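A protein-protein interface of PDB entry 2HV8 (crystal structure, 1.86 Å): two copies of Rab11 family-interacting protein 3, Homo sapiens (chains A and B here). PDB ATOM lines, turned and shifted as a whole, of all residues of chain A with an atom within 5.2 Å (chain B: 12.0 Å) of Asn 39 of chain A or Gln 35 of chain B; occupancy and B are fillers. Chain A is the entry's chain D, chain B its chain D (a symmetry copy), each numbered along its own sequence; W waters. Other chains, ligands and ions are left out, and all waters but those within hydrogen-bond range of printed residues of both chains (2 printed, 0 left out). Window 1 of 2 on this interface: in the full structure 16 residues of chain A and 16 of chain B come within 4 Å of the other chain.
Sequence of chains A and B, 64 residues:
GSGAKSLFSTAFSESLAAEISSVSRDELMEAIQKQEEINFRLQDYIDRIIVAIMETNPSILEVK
Printed residues of chain B that touch a printed residue of chain A: Gln 35, Ile 38, Asn 39, Leu 42, Gln 43 and Ile 46.
Hydrophobic or aromatic side chains of chain B within 4 Å of the printed part of chain A: Ile 38, Leu 42 and Ile 46.
Along chain B the printed residues that touch a printed residue of chain A span positions 35 to 46.
Among the printed residues, no Asp or Glu carboxylate lies within 4 Å of a Lys or Arg side-chain nitrogen of the other chain.
Water W2 bridges the side-chain amide oxygen (OD1) of Asn 39 of chain A and the side-chain amide nitrogen (NE2) of Gln 35 of chain B.
Water W1 lies within hydrogen-bond range of OD1 of Asn 39 of chain B (3.0 Å) and NE2 of Gln 35 of chain A (3.4 Å).
Gln 35 of chain A touches Asn 39 of chain B.
CG2 of Ile 38 of chain A touches ND2 of Asn 39 of chain B (3.1 Å).
CB of Asn 39 of chain A touches OE1 of Gln 35 of chain B, 3.96 Å away.
ND2 of Asn 39 of chain A touches CG2 of Ile 38 of chain B, 3.1 Å away.
Leu 42 of chain B touches Asn 39 of chain A (CD1 to O, 3.7 Å).
Asn 39 of chain B touches Leu 42 of chain A (O to CD1, 3.7 Å).
CB of Leu 42 of chain B touches CD1 of Leu 42 of chain A, 3.8 Å away.
Leu 42 of chain A touches Gln 43 of chain B (CD2 to NE2, 3.7 Å).
Leu 42 of chain A touches Ile 46 of chain B (CD2 to CD1, 3.8 Å).
Gln 43 of chain A touches Leu 42 of chain B (NE2 to CD2, 3.7 Å).
Of the printed residues of chain B, Asn 39 of chain A touches Gln 35 (3.96 Å), Ile 38 (3.1 Å) and Leu 42 (3.7 Å).
Gln 35 of chain A touches just one residue of chain B: Asn 39 (3.96 Å).
Glu 36 of chain A touches none of the printed residues of chain B.
Ile 38 of chain A touches one residue of chain B.
No residue of chain B comes within 4 Å of Phe 40 of chain A.
Gln 43 of chain A touches just one residue of chain B: Leu 42 (3.7 Å).
Of the printed residues of chain A, Ile 46 of chain B touches Leu 42.
Printed residues of chain A within 4 Å of Leu 42 of chain B: Asn 39, Leu 42 and Gln 43.
Of the printed residues of chain A, Asn 39 of chain B touches Gln 35 (3.96 Å), Ile 38 (3.1 Å) and Leu 42 (3.7 Å).
The nearest residue of chain B that does not touch Asn 39 of chain A is Asn 39 of chain B (4.9 Å).
The nearest residue of chain A that does not touch Gln 35 of chain B is Gln 35 of chain A (4.2 Å).
The nearest printed residue of chain A that does not touch Leu 42 of chain B is Ile 38 of chain A (5.6 Å).
Gln 35 of chain A touches Asn 39 of chain B, and with the chains exchanged Asn 39 of chain A touches Gln 35 of chain B.
Ile 38 of chain A touches Asn 39 of chain B, and with the chains exchanged Asn 39 of chain A touches Ile 38 of chain B.
Leu 42 of chain B touches its own counterpart, Leu 42 of chain A.
Leu 42 of chain A touches Gln 43 of chain B, and with the chains exchanged Gln 43 of chain A touches Leu 42 of chain B.
Of the 10 pairs that touch across the chains among the printed residues, 9 have their exchanged pair printed and touching as well.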
ATOM      1  N   GLN A  35      14.261  15.194 -27.509  1.00  0.00           N
ATOM      2  CA  GLN A  35      15.007  16.331 -26.962  1.00  0.00           C
ATOM      3  C   GLN A  35      14.851  16.482 -25.453  1.00  0.00           C
ATOM      4  O   GLN A  35      15.810  16.849 -24.766  1.00  0.00           O
ATOM      5  CB  GLN A  35      14.617  17.633 -27.667  1.00  0.00           C
ATOM      6  CG  GLN A  35      15.244  17.797 -29.043  1.00  0.00           C
ATOM      7  CD  GLN A  35      16.759  17.894 -28.990  1.00  0.00           C
ATOM      8  OE1 GLN A  35      17.320  18.679 -28.222  1.00  0.00           O
ATOM      9  NE2 GLN A  35      17.430  17.095 -29.816  1.00  0.00           N
ATOM     10  N   GLU A  36      13.656  16.202 -24.939  1.00  0.00           N
ATOM     11  CA  GLU A  36      13.427  16.228 -23.497  1.00  0.00           C
ATOM     12  C   GLU A  36      14.215  15.123 -22.792  1.00  0.00           C
ATOM     13  O   GLU A  36      14.782  15.353 -21.723  1.00  0.00           O
ATOM     14  CB  GLU A  36      11.936  16.137 -23.156  1.00  0.00           C
ATOM     15  CG  GLU A  36      11.642  16.376 -21.672  1.00  0.00           C
ATOM     16  CD  GLU A  36      10.166  16.512 -21.349  1.00  0.00           C
ATOM     17  OE1 GLU A  36       9.349  16.707 -22.277  1.00  0.00           O
ATOM     18  OE2 GLU A  36       9.823  16.430 -20.148  1.00  0.00           O
ATOM     19  N   GLU A  37      14.249  13.936 -23.398  1.00  0.00           N
ATOM     20  CA  GLU A  37      15.036  12.817 -22.877  1.00  0.00           C
ATOM     21  C   GLU A  37      16.519  13.178 -22.777  1.00  0.00           C
ATOM     22  O   GLU A  37      17.146  12.937 -21.746  1.00  0.00           O
ATOM     23  CB  GLU A  37      14.856  11.559 -23.735  1.00  0.00           C
ATOM     24  CG  GLU A  37      15.586  10.331 -23.193  1.00  0.00           C
ATOM     25  CD  GLU A  37      15.700   9.197 -24.204  1.00  0.00           C
ATOM     26  OE1 GLU A  37      15.042   9.258 -25.267  1.00  0.00           O
ATOM     27  OE2 GLU A  37      16.456   8.241 -23.932  1.00  0.00           O
ATOM     28  N   ILE A  38      17.069  13.760 -23.841  1.00  0.00           N
ATOM     29  CA  ILE A  38      18.478  14.150 -23.843  1.00  0.00           C
ATOM     30  C   ILE A  38      18.764  15.214 -22.775  1.00  0.00           C
ATOM     31  O   ILE A  38      19.712  15.059 -22.008  1.00  0.00           O
ATOM     32  CB  ILE A  38      18.993  14.583 -25.243  1.00  0.00           C
ATOM     33  CG1 ILE A  38      18.701  13.495 -26.282  1.00  0.00           C
ATOM     34  CG2 ILE A  38      20.498  14.833 -25.196  1.00  0.00           C
ATOM     35  CD1 ILE A  38      18.819  13.959 -27.735  1.00  0.00           C
ATOM     36  N   ASN A  39      17.935  16.263 -22.704  1.00  0.00           N
ATOM     37  CA  ASN A  39      18.072  17.295 -21.659  1.00  0.00           C
ATOM     38  C   ASN A  39      18.134  16.697 -20.265  1.00  0.00           C
ATOM     39  O   ASN A  39      19.013  17.044 -19.474  1.00  0.00           O
ATOM     40  CB  ASN A  39      16.934  18.328 -21.707  1.00  0.00           C
ATOM     41  CG  ASN A  39      16.971  19.308 -20.520  1.00  0.00           C
ATOM     42  OD1 ASN A  39      16.559  18.983 -19.398  1.00  0.00           O
ATOM     43  ND2 ASN A  39      17.456  20.513 -20.773  1.00  0.00           N
ATOM     44  N   PHE A  40      17.188  15.807 -19.974  1.00  0.00           N
ATOM     45  CA  PHE A  40      17.104  15.167 -18.670  1.00  0.00           C
ATOM     46  C   PHE A  40      18.300  14.259 -18.390  1.00  0.00           C
ATOM     47  O   PHE A  40      18.789  14.209 -17.264  1.00  0.00           O
ATOM     48  CB  PHE A  40      15.782  14.407 -18.522  1.00  0.00           C
ATOM     49  CG  PHE A  40      14.654  15.256 -17.992  1.00  0.00           C
ATOM     50  CD1 PHE A  40      14.089  16.264 -18.772  1.00  0.00           C
ATOM     51  CD2 PHE A  40      14.163  15.048 -16.708  1.00  0.00           C
ATOM     52  CE1 PHE A  40      13.045  17.050 -18.278  1.00  0.00           C
ATOM     53  CE2 PHE A  40      13.125  15.828 -16.207  1.00  0.00           C
ATOM     54  CZ  PHE A  40      12.564  16.828 -16.991  1.00  0.00           C
ATOM     55  N   ARG A  41      18.772  13.559 -19.421  1.00  0.00           N
ATOM     56  CA  ARG A  41      19.958  12.712 -19.284  1.00  0.00           C
ATOM     57  C   ARG A  41      21.218  13.538 -19.046  1.00  0.00           C
ATOM     58  O   ARG A  41      22.043  13.174 -18.207  1.00  0.00           O
ATOM     59  CB  ARG A  41      20.144  11.815 -20.510  1.00  0.00           C
ATOM     60  CG  ARG A  41      19.123  10.690 -20.602  1.00  0.00           C
ATOM     61  CD  ARG A  41      19.392   9.777 -21.806  1.00  0.00           C
ATOM     62  NE  ARG A  41      20.669   9.079 -21.688  1.00  0.00           N
ATOM     63  CZ  ARG A  41      21.643   9.123 -22.595  1.00  0.00           C
ATOM     64  NH1 ARG A  41      21.493   9.821 -23.717  1.00  0.00           N
ATOM     65  NH2 ARG A  41      22.765   8.453 -22.390  1.00  0.00           N
ATOM     66  N   LEU A  42      21.354  14.644 -19.778  1.00  0.00           N
ATOM     67  CA  LEU A  42      22.518  15.522 -19.641  1.00  0.00           C
ATOM     68  C   LEU A  42      22.535  16.224 -18.286  1.00  0.00           C
ATOM     69  O   LEU A  42      23.575  16.286 -17.631  1.00  0.00           O
ATOM     70  CB  LEU A  42      22.588  16.555 -20.775  1.00  0.00           C
ATOM     71  CG  LEU A  42      22.771  16.083 -22.226  1.00  0.00           C
ATOM     72  CD1 LEU A  42      22.953  17.284 -23.149  1.00  0.00           C
ATOM     73  CD2 LEU A  42      23.941  15.120 -22.362  1.00  0.00           C
ATOM     74  N   GLN A  43      21.383  16.741 -17.863  1.00  0.00           N
ATOM     75  CA  GLN A  43      21.307  17.398 -16.560  1.00  0.00           C
ATOM     76  C   GLN A  43      21.613  16.417 -15.432  1.00  0.00           C
ATOM     77  O   GLN A  43      22.305  16.773 -14.476  1.00  0.00           O
ATOM     78  CB  GLN A  43      19.956  18.085 -16.344  1.00  0.00           C
ATOM     79  CG  GLN A  43      19.894  18.948 -15.070  1.00  0.00           C
ATOM     80  CD  GLN A  43      20.823  20.154 -15.115  1.00  0.00           C
ATOM     81  OE1 GLN A  43      21.842  20.203 -14.416  1.00  0.00           O
ATOM     82  NE2 GLN A  43      20.481  21.126 -15.939  1.00  0.00           N
ATOM     83  N   ASP A  44      21.115  15.186 -15.547  1.00  0.00           N
ATOM     84  CA  ASP A  44      21.416  14.155 -14.551  1.00  0.00           C
ATOM     85  C   ASP A  44      22.907  13.817 -14.515  1.00  0.00           C
ATOM     86  O   ASP A  44      23.490  13.682 -13.442  1.00  0.00           O
ATOM     87  CB  ASP A  44      20.601  12.879 -14.775  1.00  0.00           C
ATOM     88  CG  ASP A  44      21.012  11.761 -13.829  1.00  0.00           C
ATOM     89  OD1 ASP A  44      20.689  11.847 -12.623  1.00  0.00           O
ATOM     90  OD2 ASP A  44      21.686  10.809 -14.283  1.00  0.00           O
ATOM     91  N   ASP B  26       4.362  29.563 -33.794  1.00  0.00           N
ATOM     92  CA  ASP B  26       5.374  30.518 -33.343  1.00  0.00           C
ATOM     93  C   ASP B  26       5.875  30.158 -31.948  1.00  0.00           C
ATOM     94  O   ASP B  26       7.074  30.221 -31.674  1.00  0.00           O
ATOM     95  CB  ASP B  26       4.813  31.935 -33.356  1.00  0.00           C
ATOM     96  N   GLU B  27       4.944  29.776 -31.075  1.00  0.00           N
ATOM     97  CA  GLU B  27       5.271  29.356 -29.713  1.00  0.00           C
ATOM     98  C   GLU B  27       5.954  27.989 -29.702  1.00  0.00           C
ATOM     99  O   GLU B  27       6.872  27.753 -28.911  1.00  0.00           O
ATOM    100  CB  GLU B  27       4.020  29.342 -28.847  1.00  0.00           C
ATOM    101  N   LEU B  28       5.504  27.100 -30.589  1.00  0.00           N
ATOM    102  CA  LEU B  28       6.107  25.775 -30.749  1.00  0.00           C
ATOM    103  C   LEU B  28       7.550  25.873 -31.242  1.00  0.00           C
ATOM    104  O   LEU B  28       8.413  25.112 -30.805  1.00  0.00           O
ATOM    105  CB  LEU B  28       5.277  24.907 -31.704  1.00  0.00           C
ATOM    106  CG  LEU B  28       3.880  24.457 -31.258  1.00  0.00           C
ATOM    107  CD1 LEU B  28       3.127  23.836 -32.430  1.00  0.00           C
ATOM    108  CD2 LEU B  28       3.940  23.484 -30.083  1.00  0.00           C
ATOM    109  N   MET B  29       7.798  26.816 -32.151  1.00  0.00           N
ATOM    110  CA  MET B  29       9.142  27.085 -32.659  1.00  0.00           C
ATOM    111  C   MET B  29      10.052  27.652 -31.572  1.00  0.00           C
ATOM    112  O   MET B  29      11.219  27.271 -31.476  1.00  0.00           O
ATOM    113  CB  MET B  29       9.082  28.033 -33.852  1.00  0.00           C
ATOM    114  N   GLU B  30       9.510  28.555 -30.756  1.00  0.00           N
ATOM    115  CA  GLU B  30      10.244  29.129 -29.626  1.00  0.00           C
ATOM    116  C   GLU B  30      10.652  28.056 -28.612  1.00  0.00           C
ATOM    117  O   GLU B  30      11.745  28.116 -28.042  1.00  0.00           O
ATOM    118  CB  GLU B  30       9.424  30.226 -28.952  1.00  0.00           C
ATOM    119  N   ALA B  31       9.770  27.081 -28.400  1.00  0.00           N
ATOM    120  CA  ALA B  31      10.049  25.956 -27.509  1.00  0.00           C
ATOM    121  C   ALA B  31      11.150  25.045 -28.061  1.00  0.00           C
ATOM    122  O   ALA B  31      11.939  24.495 -27.290  1.00  0.00           O
ATOM    123  CB  ALA B  31       8.779  25.163 -27.228  1.00  0.00           C
ATOM    124  N   ILE B  32      11.194  24.892 -29.387  1.00  0.00           N
ATOM    125  CA  ILE B  32      12.253  24.133 -30.067  1.00  0.00           C
ATOM    126  C   ILE B  32      13.617  24.786 -29.849  1.00  0.00           C
ATOM    127  O   ILE B  32      14.583  24.113 -29.477  1.00  0.00           O
ATOM    128  CB  ILE B  32      12.002  24.012 -31.604  1.00  0.00           C
ATOM    129  CG1 ILE B  32      10.710  23.245 -31.911  1.00  0.00           C
ATOM    130  CG2 ILE B  32      13.209  23.378 -32.327  1.00  0.00           C
ATOM    131  CD1 ILE B  32      10.691  21.817 -31.439  1.00  0.00           C
ATOM    132  N   GLN B  33      13.682  26.094 -30.094  1.00  0.00           N
ATOM    133  CA  GLN B  33      14.923  26.857 -29.959  1.00  0.00           C
ATOM    134  C   GLN B  33      15.430  26.868 -28.519  1.00  0.00           C
ATOM    135  O   GLN B  33      16.633  26.725 -28.283  1.00  0.00           O
ATOM    136  CB  GLN B  33      14.734  28.280 -30.475  1.00  0.00           C
ATOM    137  N   LYS B  34      14.510  27.029 -27.566  1.00  0.00           N
ATOM    138  CA  LYS B  34      14.849  27.027 -26.141  1.00  0.00           C
ATOM    139  C   LYS B  34      15.466  25.697 -25.709  1.00  0.00           C
ATOM    140  O   LYS B  34      16.468  25.682 -24.995  1.00  0.00           O
ATOM    141  CB  LYS B  34      13.624  27.351 -25.294  1.00  0.00           C
ATOM    142  N   GLN B  35      14.874  24.593 -26.162  1.00  0.00           N
ATOM    143  CA  GLN B  35      15.361  23.250 -25.833  1.00  0.00           C
ATOM    144  C   GLN B  35      16.679  22.905 -26.519  1.00  0.00           C
ATOM    145  O   GLN B  35      17.529  22.236 -25.922  1.00  0.00           O
ATOM    146  CB  GLN B  35      14.305  22.189 -26.154  1.00  0.00           C
ATOM    147  CG  GLN B  35      13.186  22.107 -25.127  1.00  0.00           C
ATOM    148  CD  GLN B  35      13.678  21.676 -23.757  1.00  0.00           C
ATOM    149  OE1 GLN B  35      14.391  20.679 -23.622  1.00  0.00           O
ATOM    150  NE2 GLN B  35      13.292  22.427 -22.728  1.00  0.00           N
ATOM    151  N   GLU B  36      16.850  23.356 -27.759  1.00  0.00           N
ATOM    152  CA  GLU B  36      18.111  23.158 -28.470  1.00  0.00           C
ATOM    153  C   GLU B  36      19.246  23.942 -27.810  1.00  0.00           C
ATOM    154  O   GLU B  36      20.360  23.432 -27.687  1.00  0.00           O
ATOM    155  CB  GLU B  36      17.989  23.518 -29.953  1.00  0.00           C
ATOM    156  CG  GLU B  36      19.223  23.122 -30.772  1.00  0.00           C
ATOM    157  CD  GLU B  36      19.040  23.263 -32.271  1.00  0.00           C
ATOM    158  OE1 GLU B  36      17.887  23.396 -32.740  1.00  0.00           O
ATOM    159  OE2 GLU B  36      20.066  23.231 -32.988  1.00  0.00           O
ATOM    160  N   GLU B  37      18.954  25.172 -27.388  1.00  0.00           N
ATOM    161  CA  GLU B  37      19.922  25.999 -26.664  1.00  0.00           C
ATOM    162  C   GLU B  37      20.390  25.312 -25.380  1.00  0.00           C
ATOM    163  O   GLU B  37      21.589  25.248 -25.115  1.00  0.00           O
ATOM    164  CB  GLU B  37      19.346  27.382 -26.342  1.00  0.00           C
ATOM    165  CG  GLU B  37      20.340  28.323 -25.661  1.00  0.00           C
ATOM    166  CD  GLU B  37      19.684  29.547 -25.033  1.00  0.00           C
ATOM    167  OE1 GLU B  37      18.485  29.796 -25.288  1.00  0.00           O
ATOM    168  OE2 GLU B  37      20.376  30.262 -24.278  1.00  0.00           O
ATOM    169  N   ILE B  38      19.446  24.796 -24.595  1.00  0.00           N
ATOM    170  CA  ILE B  38      19.790  24.113 -23.349  1.00  0.00           C
ATOM    171  C   ILE B  38      20.635  22.860 -23.615  1.00  0.00           C
ATOM    172  O   ILE B  38      21.671  22.684 -22.975  1.00  0.00           O
ATOM    173  CB  ILE B  38      18.556  23.800 -22.459  1.00  0.00           C
ATOM    174  CG1 ILE B  38      17.742  25.073 -22.205  1.00  0.00           C
ATOM    175  CG2 ILE B  38      19.006  23.223 -21.119  1.00  0.00           C
ATOM    176  CD1 ILE B  38      16.330  24.825 -21.670  1.00  0.00           C
ATOM    177  N   ASN B  39      20.218  22.019 -24.569  1.00  0.00           N
ATOM    178  CA  ASN B  39      21.004  20.833 -24.960  1.00  0.00           C
ATOM    179  C   ASN B  39      22.445  21.181 -25.288  1.00  0.00           C
ATOM    180  O   ASN B  39      23.372  20.532 -24.798  1.00  0.00           O
ATOM    181  CB  ASN B  39      20.385  20.093 -26.158  1.00  0.00           C
ATOM    182  CG  ASN B  39      21.284  18.957 -26.682  1.00  0.00           C
ATOM    183  OD1 ASN B  39      22.268  19.187 -27.398  1.00  0.00           O
ATOM    184  ND2 ASN B  39      20.935  17.730 -26.333  1.00  0.00           N
ATOM    185  N   PHE B  40      22.619  22.199 -26.127  1.00  0.00           N
ATOM    186  CA  PHE B  40      23.941  22.632 -26.553  1.00  0.00           C
ATOM    187  C   PHE B  40      24.764  23.203 -25.400  1.00  0.00           C
ATOM    188  O   PHE B  40      25.969  22.971 -25.325  1.00  0.00           O
ATOM    189  CB  PHE B  40      23.839  23.630 -27.710  1.00  0.00           C
ATOM    190  CG  PHE B  40      23.800  22.975 -29.069  1.00  0.00           C
ATOM    191  CD1 PHE B  40      22.684  22.248 -29.481  1.00  0.00           C
ATOM    192  CD2 PHE B  40      24.884  23.084 -29.932  1.00  0.00           C
ATOM    193  CE1 PHE B  40      22.650  21.642 -30.739  1.00  0.00           C
ATOM    194  CE2 PHE B  40      24.860  22.482 -31.186  1.00  0.00           C
ATOM    195  CZ  PHE B  40      23.743  21.762 -31.592  1.00  0.00           C
ATOM    196  N   ARG B  41      24.107  23.934 -24.501  1.00  0.00           N
ATOM    197  CA  ARG B  41      24.782  24.471 -23.317  1.00  0.00           C
ATOM    198  C   ARG B  41      25.208  23.364 -22.360  1.00  0.00           C
ATOM    199  O   ARG B  41      26.318  23.405 -21.827  1.00  0.00           O
ATOM    200  CB  ARG B  41      23.898  25.484 -22.587  1.00  0.00           C
ATOM    201  CG  ARG B  41      23.745  26.805 -23.327  1.00  0.00           C
ATOM    202  CD  ARG B  41      22.911  27.813 -22.524  1.00  0.00           C
ATOM    203  NE  ARG B  41      23.564  28.189 -21.274  1.00  0.00           N
ATOM    204  CZ  ARG B  41      23.012  28.074 -20.067  1.00  0.00           C
ATOM    205  NH1 ARG B  41      21.775  27.608 -19.930  1.00  0.00           N
ATOM    206  NH2 ARG B  41      23.692  28.444 -18.994  1.00  0.00           N
ATOM    207  N   LEU B  42      24.330  22.382 -22.154  1.00  0.00           N
ATOM    208  CA  LEU B  42      24.622  21.261 -21.258  1.00  0.00           C
ATOM    209  C   LEU B  42      25.730  20.371 -21.815  1.00  0.00           C
ATOM    210  O   LEU B  42      26.643  19.983 -21.085  1.00  0.00           O
ATOM    211  CB  LEU B  42      23.368  20.425 -20.965  1.00  0.00           C
ATOM    212  CG  LEU B  42      22.182  21.064 -20.224  1.00  0.00           C
ATOM    213  CD1 LEU B  42      21.121  20.010 -19.925  1.00  0.00           C
ATOM    214  CD2 LEU B  42      22.625  21.759 -18.944  1.00  0.00           C
ATOM    215  N   GLN B  43      25.657  20.058 -23.107  1.00  0.00           N
ATOM    216  CA  GLN B  43      26.698  19.240 -23.726  1.00  0.00           C
ATOM    217  C   GLN B  43      28.051  19.945 -23.678  1.00  0.00           C
ATOM    218  O   GLN B  43      29.070  19.303 -23.419  1.00  0.00           O
ATOM    219  CB  GLN B  43      26.334  18.839 -25.158  1.00  0.00           C
ATOM    220  CG  GLN B  43      27.308  17.824 -25.786  1.00  0.00           C
ATOM    221  CD  GLN B  43      27.287  16.467 -25.096  1.00  0.00           C
ATOM    222  OE1 GLN B  43      28.237  16.089 -24.399  1.00  0.00           O
ATOM    223  NE2 GLN B  43      26.207  15.731 -25.281  1.00  0.00           N
ATOM    224  N   ASP B  44      28.060  21.256 -23.909  1.00  0.00           N
ATOM    225  CA  ASP B  44      29.299  22.031 -23.812  1.00  0.00           C
ATOM    226  C   ASP B  44      29.863  22.026 -22.391  1.00  0.00           C
ATOM    227  O   ASP B  44      31.066  21.863 -22.197  1.00  0.00           O
ATOM    228  CB  ASP B  44      29.120  23.472 -24.293  1.00  0.00           C
ATOM    229  CG  ASP B  44      30.367  24.314 -24.064  1.00  0.00           C
ATOM    230  OD1 ASP B  44      31.367  24.115 -24.790  1.00  0.00           O
ATOM    231  OD2 ASP B  44      30.360  25.155 -23.136  1.00  0.00           O
ATOM    232  N   TYR B  45      28.984  22.218 -21.408  1.00  0.00           N
ATOM    233  CA  TYR B  45      29.365  22.181 -19.996  1.00  0.00           C
ATOM    234  C   TYR B  45      30.030  20.839 -19.663  1.00  0.00           C
ATOM    235  O   TYR B  45      31.088  20.798 -19.019  1.00  0.00           O
ATOM    236  CB  TYR B  45      28.121  22.411 -19.126  1.00  0.00           C
ATOM    237  CG  TYR B  45      28.398  22.627 -17.652  1.00  0.00           C
ATOM    238  CD1 TYR B  45      28.613  23.910 -17.146  1.00  0.00           C
ATOM    239  CD2 TYR B  45      28.416  21.553 -16.763  1.00  0.00           C
ATOM    240  CE1 TYR B  45      28.851  24.114 -15.790  1.00  0.00           C
ATOM    241  CE2 TYR B  45      28.656  21.746 -15.407  1.00  0.00           C
ATOM    242  CZ  TYR B  45      28.870  23.030 -14.931  1.00  0.00           C
ATOM    243  OH  TYR B  45      29.108  23.232 -13.594  1.00  0.00           O
ATOM    244  N   ILE B  46      29.411  19.752 -20.124  1.00  0.00           N
ATOM    245  CA  ILE B  46      29.946  18.397 -19.967  1.00  0.00           C
ATOM    246  C   ILE B  46      31.296  18.236 -20.674  1.00  0.00           C
ATOM    247  O   ILE B  46      32.248  17.741 -20.073  1.00  0.00           O
ATOM    248  CB  ILE B  46      28.934  17.327 -20.453  1.00  0.00           C
ATOM    249  CG1 ILE B  46      27.771  17.208 -19.458  1.00  0.00           C
ATOM    250  CG2 ILE B  46      29.609  15.958 -20.647  1.00  0.00           C
ATOM    251  CD1 ILE B  46      26.556  16.493 -20.002  1.00  0.00           C
HETATM  252  O   HOH W   1      20.755  17.524 -29.443  1.00  0.00           O
HETATM  253  O   HOH W   2      14.563  21.231 -19.842  1.00  0.00           O
